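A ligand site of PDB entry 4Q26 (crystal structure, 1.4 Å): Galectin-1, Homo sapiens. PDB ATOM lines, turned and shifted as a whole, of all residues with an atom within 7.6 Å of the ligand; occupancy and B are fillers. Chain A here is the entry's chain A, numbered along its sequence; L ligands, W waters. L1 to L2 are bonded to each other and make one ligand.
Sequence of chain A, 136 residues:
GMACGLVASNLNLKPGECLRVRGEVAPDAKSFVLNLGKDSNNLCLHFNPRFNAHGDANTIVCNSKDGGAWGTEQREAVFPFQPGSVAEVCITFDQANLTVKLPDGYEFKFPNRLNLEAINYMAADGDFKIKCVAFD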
ATOM      1  N   SER A  31     -31.744 -24.039 -23.478  1.00  0.00           N
ATOM      2  CA  SER A  31     -30.706 -23.083 -23.813  1.00  0.00           C
ATOM      3  C   SER A  31     -31.241 -22.197 -24.913  1.00  0.00           C
ATOM      4  O   SER A  31     -32.349 -22.408 -25.390  1.00  0.00           O
ATOM      5  CB  SER A  31     -29.422 -23.791 -24.281  1.00  0.00           C
ATOM      6  OG  SER A  31     -29.512 -24.288 -25.606  1.00  0.00           O
ATOM      7  N   VAL A  33     -29.515 -19.686 -28.366  1.00  0.00           N
ATOM      8  CA  VAL A  33     -28.341 -19.366 -29.128  1.00  0.00           C
ATOM      9  C   VAL A  33     -28.538 -18.073 -29.958  1.00  0.00           C
ATOM     10  O   VAL A  33     -29.587 -17.882 -30.610  1.00  0.00           O
ATOM     11  CB  VAL A  33     -28.010 -20.533 -30.128  1.00  0.00           C
ATOM     12  CG1 VAL A  33     -26.859 -20.147 -31.019  1.00  0.00           C
ATOM     13  CG2 VAL A  33     -27.705 -21.830 -29.371  1.00  0.00           C
ATOM     14  N   ASN A  35     -25.932 -16.509 -32.881  1.00  0.00           N
ATOM     15  CA  ASN A  35     -24.705 -16.717 -33.651  1.00  0.00           C
ATOM     16  C   ASN A  35     -24.402 -15.470 -34.451  1.00  0.00           C
ATOM     17  O   ASN A  35     -25.322 -14.910 -35.093  1.00  0.00           O
ATOM     18  CB  ASN A  35     -24.807 -17.903 -34.610  1.00  0.00           C
ATOM     19  CG  ASN A  35     -24.760 -19.252 -33.934  1.00  0.00           C
ATOM     20  OD1 ASN A  35     -24.192 -19.349 -32.819  1.00  0.00           O
ATOM     21  ND2 ASN A  35     -25.372 -20.260 -34.502  1.00  0.00           N
ATOM     22  N   HIS A  46     -20.528 -17.671 -31.173  1.00  0.00           N
ATOM     23  CA  HIS A  46     -21.640 -18.516 -30.816  1.00  0.00           C
ATOM     24  C   HIS A  46     -21.902 -18.187 -29.376  1.00  0.00           C
ATOM     25  O   HIS A  46     -21.035 -18.508 -28.509  1.00  0.00           O
ATOM     26  CB  HIS A  46     -21.211 -20.006 -31.030  1.00  0.00           C
ATOM     27  CG  HIS A  46     -22.150 -21.017 -30.458  1.00  0.00           C
ATOM     28  ND1 HIS A  46     -23.377 -21.319 -31.001  1.00  0.00           N
ATOM     29  CD2 HIS A  46     -21.955 -21.942 -29.471  1.00  0.00           C
ATOM     30  CE1 HIS A  46     -23.940 -22.291 -30.333  1.00  0.00           C
ATOM     31  NE2 HIS A  46     -23.102 -22.688 -29.381  1.00  0.00           N
ATOM     32  N   PHE A  47     -23.006 -17.562 -29.096  1.00  0.00           N
ATOM     33  CA  PHE A  47     -23.352 -17.114 -27.733  1.00  0.00           C
ATOM     34  C   PHE A  47     -24.462 -18.028 -27.238  1.00  0.00           C
ATOM     35  O   PHE A  47     -25.562 -17.954 -27.753  1.00  0.00           O
ATOM     36  CB  PHE A  47     -23.812 -15.650 -27.830  1.00  0.00           C
ATOM     37  CG  PHE A  47     -24.287 -15.053 -26.504  1.00  0.00           C
ATOM     38  CD1 PHE A  47     -23.344 -14.721 -25.565  1.00  0.00           C
ATOM     39  CD2 PHE A  47     -25.634 -14.918 -26.176  1.00  0.00           C
ATOM     40  CE1 PHE A  47     -23.752 -14.147 -24.342  1.00  0.00           C
ATOM     41  CE2 PHE A  47     -26.054 -14.349 -24.973  1.00  0.00           C
ATOM     42  CZ  PHE A  47     -25.084 -13.977 -24.065  1.00  0.00           C
ATOM     43  N   ASN A  48     -24.179 -18.916 -26.245  1.00  0.00           N
ATOM     44  CA  ASN A  48     -25.115 -19.967 -25.923  1.00  0.00           C
ATOM     45  C   ASN A  48     -25.352 -20.036 -24.417  1.00  0.00           C
ATOM     46  O   ASN A  48     -24.760 -20.905 -23.749  1.00  0.00           O
ATOM     47  CB  ASN A  48     -24.544 -21.301 -26.479  1.00  0.00           C
ATOM     48  CG  ASN A  48     -25.393 -22.511 -26.256  1.00  0.00           C
ATOM     49  OD1 ASN A  48     -24.809 -23.615 -26.231  1.00  0.00           O
ATOM     50  ND2 ASN A  48     -26.704 -22.399 -26.138  1.00  0.00           N
ATOM     51  N   ARG A  50     -26.918 -21.593 -21.411  1.00  0.00           N
ATOM     52  CA  ARG A  50     -27.475 -22.900 -21.173  1.00  0.00           C
ATOM     53  C   ARG A  50     -28.143 -22.879 -19.777  1.00  0.00           C
ATOM     54  O   ARG A  50     -27.493 -22.730 -18.753  1.00  0.00           O
ATOM     55  CB  ARG A  50     -26.389 -23.980 -21.225  1.00  0.00           C
ATOM     56  CG  ARG A  50     -25.669 -24.028 -22.597  1.00  0.00           C
ATOM     57  CD  ARG A  50     -24.550 -25.053 -22.653  1.00  0.00           C
ATOM     58  NE  ARG A  50     -24.004 -25.106 -23.997  1.00  0.00           N
ATOM     59  CZ  ARG A  50     -22.979 -25.870 -24.345  1.00  0.00           C
ATOM     60  NH1 ARG A  50     -22.382 -26.649 -23.431  1.00  0.00           N
ATOM     61  NH2 ARG A  50     -22.532 -25.921 -25.572  1.00  0.00           N
ATOM     62  N   ALA A  53     -28.222 -27.823 -20.308  1.00  0.00           N
ATOM     63  CA  ALA A  53     -27.929 -28.414 -21.599  1.00  0.00           C
ATOM     64  C   ALA A  53     -26.479 -28.807 -21.720  1.00  0.00           C
ATOM     65  O   ALA A  53     -25.595 -28.066 -21.306  1.00  0.00           O
ATOM     66  CB  ALA A  53     -28.283 -27.417 -22.718  1.00  0.00           C
ATOM     67  N   HIS A  54     -26.253 -29.959 -22.344  1.00  0.00           N
ATOM     68  CA  HIS A  54     -24.898 -30.439 -22.678  1.00  0.00           C
ATOM     69  C   HIS A  54     -23.969 -30.474 -21.444  1.00  0.00           C
ATOM     70  O   HIS A  54     -22.739 -30.297 -21.566  1.00  0.00           O
ATOM     71  CB  HIS A  54     -24.272 -29.586 -23.787  1.00  0.00           C
ATOM     72  CG  HIS A  54     -25.200 -29.263 -24.934  1.00  0.00           C
ATOM     73  ND1 HIS A  54     -25.645 -30.225 -25.827  1.00  0.00           N
ATOM     74  CD2 HIS A  54     -25.729 -28.084 -25.347  1.00  0.00           C
ATOM     75  CE1 HIS A  54     -26.428 -29.646 -26.726  1.00  0.00           C
ATOM     76  NE2 HIS A  54     -26.483 -28.350 -26.469  1.00  0.00           N
ATOM     77  N   GLY A  55     -24.557 -30.723 -20.270  1.00  0.00           N
ATOM     78  CA  GLY A  55     -23.771 -30.813 -19.064  1.00  0.00           C
ATOM     79  C   GLY A  55     -23.627 -29.547 -18.242  1.00  0.00           C
ATOM     80  O   GLY A  55     -23.005 -29.562 -17.179  1.00  0.00           O
ATOM     81  N   ASP A  56     -24.149 -28.444 -18.756  1.00  0.00           N
ATOM     82  CA  ASP A  56     -24.070 -27.115 -18.087  1.00  0.00           C
ATOM     83  C   ASP A  56     -25.409 -26.672 -17.529  1.00  0.00           C
ATOM     84  O   ASP A  56     -26.412 -26.811 -18.199  1.00  0.00           O
ATOM     85  CB  ASP A  56     -23.586 -26.032 -19.072  1.00  0.00           C
ATOM     86  CG  ASP A  56     -22.156 -26.269 -19.560  1.00  0.00           C
ATOM     87  OD1 ASP A  56     -21.234 -26.125 -18.731  1.00  0.00           O
ATOM     88  OD2 ASP A  56     -21.926 -26.615 -20.725  1.00  0.00           O
ATOM     89  N   VAL A  61     -22.046 -20.338 -22.458  1.00  0.00           N
ATOM     90  CA  VAL A  61     -20.957 -20.916 -23.217  1.00  0.00           C
ATOM     91  C   VAL A  61     -20.784 -20.104 -24.502  1.00  0.00           C
ATOM     92  O   VAL A  61     -21.749 -19.861 -25.174  1.00  0.00           O
ATOM     93  CB  VAL A  61     -21.253 -22.409 -23.570  1.00  0.00           C
ATOM     94  CG1 VAL A  61     -20.164 -22.979 -24.447  1.00  0.00           C
ATOM     95  CG2 VAL A  61     -21.407 -23.242 -22.276  1.00  0.00           C
ATOM     96  N   CYS A  62     -19.543 -19.667 -24.770  1.00  0.00           N
ATOM     97  CA  CYS A  62     -19.241 -19.004 -26.017  1.00  0.00           C
ATOM     98  C   CYS A  62     -18.186 -19.761 -26.764  1.00  0.00           C
ATOM     99  O   CYS A  62     -17.316 -20.433 -26.186  1.00  0.00           O
ATOM    100  CB  CYS A  62     -18.763 -17.570 -25.797  1.00  0.00           C
ATOM    101  SG  CYS A  62     -19.935 -16.455 -25.080  1.00  0.00           S
ATOM    102  N   ASN A  63     -18.289 -19.722 -28.113  1.00  0.00           N
ATOM    103  CA  ASN A  63     -17.273 -20.354 -28.946  1.00  0.00           C
ATOM    104  C   ASN A  63     -17.205 -19.636 -30.306  1.00  0.00           C
ATOM    105  O   ASN A  63     -18.037 -18.761 -30.597  1.00  0.00           O
ATOM    106  CB  ASN A  63     -17.559 -21.846 -29.077  1.00  0.00           C
ATOM    107  CG  ASN A  63     -16.296 -22.682 -29.295  1.00  0.00           C
ATOM    108  OD1 ASN A  63     -15.207 -22.176 -29.577  1.00  0.00           O
ATOM    109  ND2 ASN A  63     -16.507 -24.002 -29.232  1.00  0.00           N
ATOM    110  N   SER A  64     -16.154 -20.005 -31.050  1.00  0.00           N
ATOM    111  CA  SER A  64     -16.032 -19.646 -32.449  1.00  0.00           C
ATOM    112  C   SER A  64     -16.246 -20.892 -33.273  1.00  0.00           C
ATOM    113  O   SER A  64     -16.244 -22.050 -32.789  1.00  0.00           O
ATOM    114  CB  SER A  64     -14.632 -19.092 -32.739  1.00  0.00           C
ATOM    115  OG  SER A  64     -13.648 -20.047 -32.324  1.00  0.00           O
ATOM    116  N   LYS A  65     -16.443 -20.649 -34.569  1.00  0.00           N
ATOM    117  CA  LYS A  65     -16.503 -21.744 -35.533  1.00  0.00           C
ATOM    118  C   LYS A  65     -15.821 -21.293 -36.793  1.00  0.00           C
ATOM    119  O   LYS A  65     -16.052 -20.210 -37.307  1.00  0.00           O
ATOM    120  CB  LYS A  65     -17.961 -22.150 -35.790  1.00  0.00           C
ATOM    121  CG  LYS A  65     -18.149 -23.429 -36.549  1.00  0.00           C
ATOM    122  CD  LYS A  65     -19.644 -23.666 -36.822  1.00  0.00           C
ATOM    123  CE  LYS A  65     -20.000 -24.991 -36.170  1.00  0.00           C
ATOM    124  NZ  LYS A  65     -21.378 -25.476 -36.416  1.00  0.00           N
ATOM    125  N   TRP A  70     -15.715 -26.189 -34.542  1.00  0.00           N
ATOM    126  CA  TRP A  70     -15.787 -25.465 -33.304  1.00  0.00           C
ATOM    127  C   TRP A  70     -14.409 -25.233 -32.746  1.00  0.00           C
ATOM    128  O   TRP A  70     -13.521 -26.151 -32.720  1.00  0.00           O
ATOM    129  CB  TRP A  70     -16.560 -26.243 -32.242  1.00  0.00           C
ATOM    130  CG  TRP A  70     -18.026 -26.360 -32.456  1.00  0.00           C
ATOM    131  CD1 TRP A  70     -18.752 -27.487 -32.649  1.00  0.00           C
ATOM    132  CD2 TRP A  70     -18.982 -25.265 -32.481  1.00  0.00           C
ATOM    133  NE1 TRP A  70     -20.089 -27.204 -32.777  1.00  0.00           N
ATOM    134  CE2 TRP A  70     -20.263 -25.847 -32.698  1.00  0.00           C
ATOM    135  CE3 TRP A  70     -18.872 -23.879 -32.364  1.00  0.00           C
ATOM    136  CZ2 TRP A  70     -21.415 -25.084 -32.804  1.00  0.00           C
ATOM    137  CZ3 TRP A  70     -20.044 -23.117 -32.430  1.00  0.00           C
ATOM    138  CH2 TRP A  70     -21.291 -23.724 -32.646  1.00  0.00           C
ATOM    139  N   GLY A  71     -14.214 -24.066 -32.182  1.00  0.00           N
ATOM    140  CA  GLY A  71     -13.012 -23.785 -31.424  1.00  0.00           C
ATOM    141  C   GLY A  71     -13.038 -24.199 -29.957  1.00  0.00           C
ATOM    142  O   GLY A  71     -13.815 -25.039 -29.529  1.00  0.00           O
ATOM    143  N   THR A  72     -12.214 -23.532 -29.177  1.00  0.00           N
ATOM    144  CA  THR A  72     -12.234 -23.762 -27.715  1.00  0.00           C
ATOM    145  C   THR A  72     -13.224 -22.898 -26.985  1.00  0.00           C
ATOM    146  O   THR A  72     -13.197 -21.652 -27.105  1.00  0.00           O
ATOM    147  CB  THR A  72     -10.840 -23.542 -27.120  1.00  0.00           C
ATOM    148  OG1 THR A  72      -9.928 -24.372 -27.836  1.00  0.00           O
ATOM    149  CG2 THR A  72     -10.799 -23.871 -25.695  1.00  0.00           C
ATOM    150  N   GLU A  73     -14.110 -23.540 -26.241  1.00  0.00           N
ATOM    151  CA  GLU A  73     -15.132 -22.825 -25.498  1.00  0.00           C
ATOM    152  C   GLU A  73     -14.597 -21.923 -24.430  1.00  0.00           C
ATOM    153  O   GLU A  73     -13.489 -22.159 -23.885  1.00  0.00           O
ATOM    154  CB  GLU A  73     -16.130 -23.776 -24.824  1.00  0.00           C
ATOM    155  CG  GLU A  73     -16.862 -24.633 -25.830  1.00  0.00           C
ATOM    156  CD  GLU A  73     -17.726 -25.710 -25.209  1.00  0.00           C
ATOM    157  OE1 GLU A  73     -17.488 -26.058 -24.023  1.00  0.00           O
ATOM    158  OE2 GLU A  73     -18.536 -26.306 -25.947  1.00  0.00           O
ATOM    159  N   GLN A  74     -15.356 -20.888 -24.134  1.00  0.00           N
ATOM    160  CA  GLN A  74     -15.146 -20.016 -22.980  1.00  0.00           C
ATOM    161  C   GLN A  74     -16.451 -20.014 -22.205  1.00  0.00           C
ATOM    162  O   GLN A  74     -17.514 -19.936 -22.791  1.00  0.00           O
ATOM    163  CB  GLN A  74     -14.827 -18.593 -23.446  1.00  0.00           C
ATOM    164  CG  GLN A  74     -14.539 -17.562 -22.378  1.00  0.00           C
ATOM    165  CD  GLN A  74     -14.175 -16.204 -22.966  1.00  0.00           C
ATOM    166  OE1 GLN A  74     -13.128 -16.047 -23.573  1.00  0.00           O
ATOM    167  NE2 GLN A  74     -15.048 -15.209 -22.762  1.00  0.00           N
ATOM    168  N   ARG A  75     -16.364 -20.005 -20.873  1.00  0.00           N
ATOM    169  CA  ARG A  75     -17.540 -19.970 -20.023  1.00  0.00           C
ATOM    170  C   ARG A  75     -17.522 -18.760 -19.132  1.00  0.00           C
ATOM    171  O   ARG A  75     -16.478 -18.369 -18.623  1.00  0.00           O
ATOM    172  CB  ARG A  75     -17.639 -21.261 -19.158  1.00  0.00           C
ATOM    173  CG  ARG A  75     -18.188 -22.458 -19.955  1.00  0.00           C
ATOM    174  CD  ARG A  75     -17.973 -23.836 -19.202  1.00  0.00           C
ATOM    175  NE  ARG A  75     -18.758 -24.888 -19.845  1.00  0.00           N
ATOM    176  CZ  ARG A  75     -18.384 -25.409 -21.004  1.00  0.00           C
ATOM    177  NH1 ARG A  75     -17.238 -25.040 -21.543  1.00  0.00           N
ATOM    178  NH2 ARG A  75     -19.146 -26.293 -21.625  1.00  0.00           N
HETATM  179  C1  LIG L   1     -18.392 -31.183 -24.920  1.00  0.00           C
HETATM  180  C2  LIG L   1     -18.625 -29.675 -24.610  1.00  0.00           C
HETATM  181  C3  LIG L   1     -19.997 -29.308 -25.010  1.00  0.00           C
HETATM  182  C4  LIG L   1     -20.136 -29.531 -26.448  1.00  0.00           C
HETATM  183  C5  LIG L   1     -19.919 -31.049 -26.746  1.00  0.00           C
HETATM  184  C6  LIG L   1     -20.016 -31.383 -28.239  1.00  0.00           C
HETATM  185  C7  LIG L   1     -17.240 -29.147 -22.733  1.00  0.00           C
HETATM  186  C8  LIG L   1     -17.222 -28.984 -21.214  1.00  0.00           C
HETATM  187  O1  LIG L   1     -18.617 -31.394 -26.348  1.00  0.00           O
HETATM  188  O2  LIG L   1     -20.180 -27.871 -24.673  1.00  0.00           O
HETATM  189  O3  LIG L   1     -21.479 -29.170 -26.855  1.00  0.00           O
HETATM  190  O4  LIG L   1     -18.988 -30.647 -28.927  1.00  0.00           O
HETATM  191  O5  LIG L   1     -16.219 -28.975 -23.421  1.00  0.00           O
HETATM  192  N1  LIG L   1     -18.415 -29.479 -23.189  1.00  0.00           N
HETATM  193  O6  LIG L   1     -19.253 -32.020 -24.195  1.00  0.00           O
HETATM  194  C1  LG2 L   2     -21.586 -28.387 -28.083  1.00  0.00           C
HETATM  195  C2  LG2 L   2     -23.002 -28.233 -28.462  1.00  0.00           C
HETATM  196  C3  LG2 L   2     -23.132 -27.282 -29.703  1.00  0.00           C
HETATM  197  C4  LG2 L   2     -22.471 -25.991 -29.410  1.00  0.00           C
HETATM  198  C5  LG2 L   2     -21.009 -26.213 -29.090  1.00  0.00           C
HETATM  199  C6  LG2 L   2     -20.175 -25.047 -28.762  1.00  0.00           C
HETATM  200  O1  LG2 L   2     -23.644 -29.489 -28.711  1.00  0.00           O
HETATM  201  O2  LG2 L   2     -24.527 -27.149 -29.905  1.00  0.00           O
HETATM  202  O3  LG2 L   2     -23.160 -25.257 -28.380  1.00  0.00           O
HETATM  203  O4  LG2 L   2     -20.977 -27.142 -27.854  1.00  0.00           O
HETATM  204  O5  LG2 L   2     -18.816 -25.319 -28.446  1.00  0.00           O
HETATM  205  O   HOH W   1     -17.373 -27.858 -28.991  1.00  0.00           O
HETATM  206  O   HOH W   2     -26.055 -29.267 -30.552  1.00  0.00           O
HETATM  207  O   HOH W   3     -23.271 -31.832 -27.300  1.00  0.00           O
HETATM  208  O   HOH W   4     -14.341 -30.684 -24.464  1.00  0.00           O
HETATM  209  O   HOH W   5     -14.097 -27.094 -23.498  1.00  0.00           O
HETATM  210  O   HOH W   6     -22.264 -32.813 -23.714  1.00  0.00           O
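CE1 of His 54 touches O1 of LG2 L2, at 3.4 Å. CZ2 of Trp 70 touches C4 of LG2 L2, 3.7 Å away. NH2 of Arg 75 touches C8 of LIG L1, at 3.3 Å.
Water W3 bridges O1 of LG2 L2 (2.8 Å) and ND1 of His 54 (3.2 Å). Water W6 lies within hydrogen-bond range of O6 of LIG L1 (3.2 Å) and O of His 54 (3.3 Å).
The guanidinium group of Arg 50 lies within hydrogen-bond range of an oxygen (O2) of LIG L1. A ring nitrogen (NE2) of His 46 is in hydrogen-bond range of an oxygen (O3) of LG2 L2 (2.8 Å). The side-chain amide oxygen (OD1) of Asn 48 sits at hydrogen-bond distance from an oxygen (O3) of LG2 L2 (3.2 Å). The side-chain amide nitrogen of Asn 63 is in hydrogen-bond range of an oxygen (O5) of LG2 L2. OE2 of Glu 73 sits at hydrogen-bond distance from O2 of LIG L1, 2.6 Å away.
The side-chain amide oxygen of Asn 63 lies close to the backbone carbonyl oxygen of Thr 72 (3.2 Å). O of Asn 63 sits at hydrogen-bond distance from N of His 46. The side-chain carboxylate of Asp 56 is in salt-bridge range of the guanidinium group of Arg 75, 2.9 Å away. The side-chain amide nitrogen (ND2) of Asn 63 sits at hydrogen-bond distance from the backbone carbonyl oxygen (O) of Gly 71 (2.9 Å). ND1 of His 46 lies within hydrogen-bond range of OD1 of Asn 35. The guanidinium group of Arg 50 is in hydrogen-bond range of the side-chain amide oxygen of Asn 48, 2.8 Å away. The side-chain hydroxyl of Ser 31 lies within hydrogen-bond range of the side-chain amide nitrogen of Asn 48 (3.4 Å). NH1 of Arg 50 lies within salt-bridge range of OD2 of Asp 56 (2.7 Å).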
